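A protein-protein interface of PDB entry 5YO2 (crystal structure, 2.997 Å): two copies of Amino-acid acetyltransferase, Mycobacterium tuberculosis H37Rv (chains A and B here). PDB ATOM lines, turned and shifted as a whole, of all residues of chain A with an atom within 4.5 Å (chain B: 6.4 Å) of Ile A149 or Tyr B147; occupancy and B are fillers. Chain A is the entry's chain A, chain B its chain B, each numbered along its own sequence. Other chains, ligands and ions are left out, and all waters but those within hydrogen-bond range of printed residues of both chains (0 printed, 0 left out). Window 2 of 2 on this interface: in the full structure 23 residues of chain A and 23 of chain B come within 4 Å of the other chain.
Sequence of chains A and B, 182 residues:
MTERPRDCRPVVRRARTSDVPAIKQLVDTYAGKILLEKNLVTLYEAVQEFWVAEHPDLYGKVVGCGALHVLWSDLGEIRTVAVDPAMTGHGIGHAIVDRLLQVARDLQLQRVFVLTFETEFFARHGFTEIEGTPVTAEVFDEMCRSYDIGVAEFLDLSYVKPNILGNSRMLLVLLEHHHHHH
Tyr A147 touches Ile B149, and with the chains exchanged Ile A149 touches Tyr B147.
Of the 2 pairs that touch across the chains among the printed residues, 2 have their exchanged pair printed and touching as well.
Printed residues of chain A that touch a printed residue of chain B: Tyr A147 and Ile A149.
Hydrophobic or aromatic side chains of chain A that line the printed part of chain B: Tyr A147 and Ile A149.
Along chain B the printed residues that touch a printed residue of chain A span positions 147 to 149.
Among the printed residues, no Asp or Glu carboxylate lies within 4 Å of a Lys or Arg side-chain nitrogen of the other chain.
Printed residues of chain B within 4 Å of Tyr A147: Ile B149 (3.7 Å).
Ile A149 touches one residue of chain B.
Val A160 touches none of the printed residues of chain B.
Tyr B147 touches just one residue of chain A: Ile A149 (3.9 Å).
Printed residues of chain A within 4 Å of Ile B149: Tyr A147 (3.7 Å).
The nearest residue of chain A that does not touch Tyr B147 is Tyr A147 (4.2 Å).
The nearest printed residue of chain B that does not touch Tyr A147 is Tyr B147 (4.2 Å).
Among the printed residues, pairs that only touch across the chains: Tyr A147 with Ile B149 (3.7 Å) and Ile A149 with Tyr B147 (3.9 Å).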
ATOM      1  N   LEU A  36      -7.229   9.193 -17.255  1.00  0.00           N
ATOM      2  CA  LEU A  36      -7.480   9.359 -15.832  1.00  0.00           C
ATOM      3  C   LEU A  36      -7.800  10.822 -15.558  1.00  0.00           C
ATOM      4  O   LEU A  36      -6.998  11.706 -15.878  1.00  0.00           O
ATOM      5  CB  LEU A  36      -6.261   8.910 -15.031  1.00  0.00           C
ATOM      6  CG  LEU A  36      -6.345   8.973 -13.505  1.00  0.00           C
ATOM      7  CD1 LEU A  36      -7.608   8.294 -12.985  1.00  0.00           C
ATOM      8  CD2 LEU A  36      -5.100   8.348 -12.892  1.00  0.00           C
ATOM      9  N   TYR A 147       0.497   8.657  -3.267  1.00  0.00           N
ATOM     10  CA  TYR A 147      -0.867   9.170  -3.304  1.00  0.00           C
ATOM     11  C   TYR A 147      -1.378   9.383  -4.723  1.00  0.00           C
ATOM     12  O   TYR A 147      -2.498   9.876  -4.893  1.00  0.00           O
ATOM     13  CB  TYR A 147      -0.961  10.490  -2.525  1.00  0.00           C
ATOM     14  CG  TYR A 147      -0.656  10.370  -1.046  1.00  0.00           C
ATOM     15  CD1 TYR A 147      -1.146   9.304  -0.300  1.00  0.00           C
ATOM     16  CD2 TYR A 147       0.118  11.323  -0.395  1.00  0.00           C
ATOM     17  CE1 TYR A 147      -0.876   9.189   1.050  1.00  0.00           C
ATOM     18  CE2 TYR A 147       0.394  11.216   0.958  1.00  0.00           C
ATOM     19  CZ  TYR A 147      -0.106  10.147   1.675  1.00  0.00           C
ATOM     20  OH  TYR A 147       0.165  10.033   3.021  1.00  0.00           O
ATOM     21  N   ASP A 148      -0.594   9.025  -5.737  1.00  0.00           N
ATOM     22  CA  ASP A 148      -0.963   9.265  -7.126  1.00  0.00           C
ATOM     23  C   ASP A 148      -1.666   8.036  -7.693  1.00  0.00           C
ATOM     24  O   ASP A 148      -1.161   6.916  -7.579  1.00  0.00           O
ATOM     25  CB  ASP A 148       0.273   9.604  -7.959  1.00  0.00           C
ATOM     26  CG  ASP A 148      -0.070   9.970  -9.393  1.00  0.00           C
ATOM     27  OD1 ASP A 148      -0.562   9.092 -10.134  1.00  0.00           O
ATOM     28  OD2 ASP A 148       0.141  11.139  -9.776  1.00  0.00           O
ATOM     29  N   ILE A 149      -2.833   8.256  -8.301  1.00  0.00           N
ATOM     30  CA  ILE A 149      -3.623   7.143  -8.818  1.00  0.00           C
ATOM     31  C   ILE A 149      -2.931   6.508 -10.017  1.00  0.00           C
ATOM     32  O   ILE A 149      -2.956   5.282 -10.185  1.00  0.00           O
ATOM     33  CB  ILE A 149      -5.045   7.619  -9.170  1.00  0.00           C
ATOM     34  CG1 ILE A 149      -5.764   8.121  -7.914  1.00  0.00           C
ATOM     35  CG2 ILE A 149      -5.839   6.494  -9.841  1.00  0.00           C
ATOM     36  CD1 ILE A 149      -7.109   8.771  -8.190  1.00  0.00           C
ATOM     37  N   GLY A 150      -2.311   7.324 -10.873  1.00  0.00           N
ATOM     38  CA  GLY A 150      -1.615   6.783 -12.027  1.00  0.00           C
ATOM     39  C   GLY A 150      -0.527   5.797 -11.654  1.00  0.00           C
ATOM     40  O   GLY A 150      -0.258   4.850 -12.398  1.00  0.00           O
ATOM     41  N   VAL A 151       0.113   6.001 -10.501  1.00  0.00           N
ATOM     42  CA  VAL A 151       1.099   5.039 -10.020  1.00  0.00           C
ATOM     43  C   VAL A 151       0.418   3.732  -9.637  1.00  0.00           C
ATOM     44  O   VAL A 151       0.938   2.643  -9.906  1.00  0.00           O
ATOM     45  CB  VAL A 151       1.891   5.635  -8.842  1.00  0.00           C
ATOM     46  CG1 VAL A 151       2.863   4.608  -8.268  1.00  0.00           C
ATOM     47  CG2 VAL A 151       2.631   6.886  -9.282  1.00  0.00           C
ATOM     48  N   ALA A 152      -0.756   3.817  -9.009  1.00  0.00           N
ATOM     49  CA  ALA A 152      -1.473   2.612  -8.613  1.00  0.00           C
ATOM     50  C   ALA A 152      -1.863   1.782  -9.827  1.00  0.00           C
ATOM     51  O   ALA A 152      -1.857   0.547  -9.774  1.00  0.00           O
ATOM     52  CB  ALA A 152      -2.713   2.987  -7.802  1.00  0.00           C
ATOM     53  N   GLU A 153      -2.214   2.444 -10.931  1.00  0.00           N
ATOM     54  CA  GLU A 153      -2.530   1.725 -12.159  1.00  0.00           C
ATOM     55  C   GLU A 153      -1.292   1.068 -12.754  1.00  0.00           C
ATOM     56  O   GLU A 153      -1.393   0.004 -13.376  1.00  0.00           O
ATOM     57  CB  GLU A 153      -3.168   2.679 -13.164  1.00  0.00           C
ATOM     58  CG  GLU A 153      -4.546   3.152 -12.742  1.00  0.00           C
ATOM     59  CD  GLU A 153      -5.174   4.089 -13.748  1.00  0.00           C
ATOM     60  OE1 GLU A 153      -6.376   4.400 -13.602  1.00  0.00           O
ATOM     61  OE2 GLU A 153      -4.466   4.520 -14.684  1.00  0.00           O
ATOM     62  N   VAL A 160      -8.082  -0.208  -8.578  1.00  0.00           N
ATOM     63  CA  VAL A 160      -8.155   0.514  -9.845  1.00  0.00           C
ATOM     64  C   VAL A 160      -8.340  -0.410 -11.035  1.00  0.00           C
ATOM     65  O   VAL A 160      -8.581   0.083 -12.149  1.00  0.00           O
ATOM     66  CB  VAL A 160      -6.909   1.402 -10.059  1.00  0.00           C
ATOM     67  CG1 VAL A 160      -6.674   2.295  -8.845  1.00  0.00           C
ATOM     68  CG2 VAL A 160      -5.674   0.552 -10.354  1.00  0.00           C
ATOM     69  N   MET B 143      -9.263  23.895  -4.327  1.00  0.00           N
ATOM     70  CA  MET B 143      -8.054  23.317  -3.755  1.00  0.00           C
ATOM     71  C   MET B 143      -8.350  22.254  -2.710  1.00  0.00           C
ATOM     72  O   MET B 143      -7.495  21.395  -2.466  1.00  0.00           O
ATOM     73  CB  MET B 143      -7.169  24.398  -3.137  1.00  0.00           C
ATOM     74  CG  MET B 143      -6.590  25.363  -4.149  1.00  0.00           C
ATOM     75  SD  MET B 143      -5.177  26.248  -3.474  1.00  0.00           S
ATOM     76  CE  MET B 143      -5.695  27.939  -3.674  1.00  0.00           C
ATOM     77  N   CYS B 144      -9.526  22.292  -2.079  1.00  0.00           N
ATOM     78  CA  CYS B 144      -9.911  21.212  -1.181  1.00  0.00           C
ATOM     79  C   CYS B 144      -9.846  19.860  -1.879  1.00  0.00           C
ATOM     80  O   CYS B 144      -9.721  18.829  -1.209  1.00  0.00           O
ATOM     81  CB  CYS B 144     -11.324  21.447  -0.641  1.00  0.00           C
ATOM     82  SG  CYS B 144     -11.391  22.303   0.952  1.00  0.00           S
ATOM     83  N   ARG B 145      -9.923  19.848  -3.209  1.00  0.00           N
ATOM     84  CA  ARG B 145      -9.954  18.631  -4.008  1.00  0.00           C
ATOM     85  C   ARG B 145      -8.570  18.024  -4.220  1.00  0.00           C
ATOM     86  O   ARG B 145      -8.448  17.038  -4.955  1.00  0.00           O
ATOM     87  CB  ARG B 145     -10.588  18.940  -5.367  1.00  0.00           C
ATOM     88  CG  ARG B 145     -11.993  19.510  -5.280  1.00  0.00           C
ATOM     89  CD  ARG B 145     -12.766  19.330  -6.578  1.00  0.00           C
ATOM     90  NE  ARG B 145     -14.060  20.011  -6.530  1.00  0.00           N
ATOM     91  CZ  ARG B 145     -15.231  19.420  -6.297  1.00  0.00           C
ATOM     92  NH1 ARG B 145     -15.304  18.110  -6.097  1.00  0.00           N
ATOM     93  NH2 ARG B 145     -16.341  20.147  -6.272  1.00  0.00           N
ATOM     94  N   SER B 146      -7.537  18.578  -3.594  1.00  0.00           N
ATOM     95  CA  SER B 146      -6.175  18.129  -3.833  1.00  0.00           C
ATOM     96  C   SER B 146      -5.847  16.900  -2.996  1.00  0.00           C
ATOM     97  O   SER B 146      -6.348  16.726  -1.882  1.00  0.00           O
ATOM     98  CB  SER B 146      -5.185  19.250  -3.511  1.00  0.00           C
ATOM     99  OG  SER B 146      -3.848  18.821  -3.698  1.00  0.00           O
ATOM    100  N   TYR B 147      -4.997  16.040  -3.551  1.00  0.00           N
ATOM    101  CA  TYR B 147      -4.454  14.904  -2.822  1.00  0.00           C
ATOM    102  C   TYR B 147      -3.139  15.239  -2.129  1.00  0.00           C
ATOM    103  O   TYR B 147      -2.546  14.360  -1.495  1.00  0.00           O
ATOM    104  CB  TYR B 147      -4.222  13.726  -3.774  1.00  0.00           C
ATOM    105  CG  TYR B 147      -5.456  13.237  -4.498  1.00  0.00           C
ATOM    106  CD1 TYR B 147      -6.680  13.126  -3.851  1.00  0.00           C
ATOM    107  CD2 TYR B 147      -5.389  12.883  -5.838  1.00  0.00           C
ATOM    108  CE1 TYR B 147      -7.804  12.678  -4.524  1.00  0.00           C
ATOM    109  CE2 TYR B 147      -6.500  12.435  -6.516  1.00  0.00           C
ATOM    110  CZ  TYR B 147      -7.704  12.333  -5.859  1.00  0.00           C
ATOM    111  OH  TYR B 147      -8.805  11.883  -6.549  1.00  0.00           O
ATOM    112  N   ASP B 148      -2.676  16.481  -2.231  1.00  0.00           N
ATOM    113  CA  ASP B 148      -1.379  16.875  -1.703  1.00  0.00           C
ATOM    114  C   ASP B 148      -1.543  17.444  -0.298  1.00  0.00           C
ATOM    115  O   ASP B 148      -2.365  18.338  -0.074  1.00  0.00           O
ATOM    116  CB  ASP B 148      -0.721  17.902  -2.626  1.00  0.00           C
ATOM    117  CG  ASP B 148       0.688  18.256  -2.199  1.00  0.00           C
ATOM    118  OD1 ASP B 148       1.564  17.368  -2.245  1.00  0.00           O
ATOM    119  OD2 ASP B 148       0.923  19.423  -1.823  1.00  0.00           O
ATOM    120  N   ILE B 149      -0.751  16.922   0.641  1.00  0.00           N
ATOM    121  CA  ILE B 149      -0.874  17.330   2.037  1.00  0.00           C
ATOM    122  C   ILE B 149      -0.386  18.761   2.228  1.00  0.00           C
ATOM    123  O   ILE B 149      -0.956  19.525   3.016  1.00  0.00           O
ATOM    124  CB  ILE B 149      -0.112  16.343   2.941  1.00  0.00           C
ATOM    125  CG1 ILE B 149      -0.719  14.943   2.803  1.00  0.00           C
ATOM    126  CG2 ILE B 149      -0.142  16.819   4.397  1.00  0.00           C
ATOM    127  CD1 ILE B 149       0.056  13.853   3.509  1.00  0.00           C
ATOM    128  N   TYR B 159      -7.902  18.309   9.329  1.00  0.00           N
ATOM    129  CA  TYR B 159      -7.203  17.057   9.591  1.00  0.00           C
ATOM    130  C   TYR B 159      -5.683  17.190   9.572  1.00  0.00           C
ATOM    131  O   TYR B 159      -4.997  16.232   9.942  1.00  0.00           O
ATOM    132  CB  TYR B 159      -7.661  15.992   8.589  1.00  0.00           C
ATOM    133  CG  TYR B 159      -7.188  16.201   7.169  1.00  0.00           C
ATOM    134  CD1 TYR B 159      -5.969  15.699   6.737  1.00  0.00           C
ATOM    135  CD2 TYR B 159      -7.974  16.890   6.254  1.00  0.00           C
ATOM    136  CE1 TYR B 159      -5.541  15.886   5.435  1.00  0.00           C
ATOM    137  CE2 TYR B 159      -7.556  17.082   4.951  1.00  0.00           C
ATOM    138  CZ  TYR B 159      -6.338  16.578   4.547  1.00  0.00           C
ATOM    139  OH  TYR B 159      -5.916  16.766   3.249  1.00  0.00           O
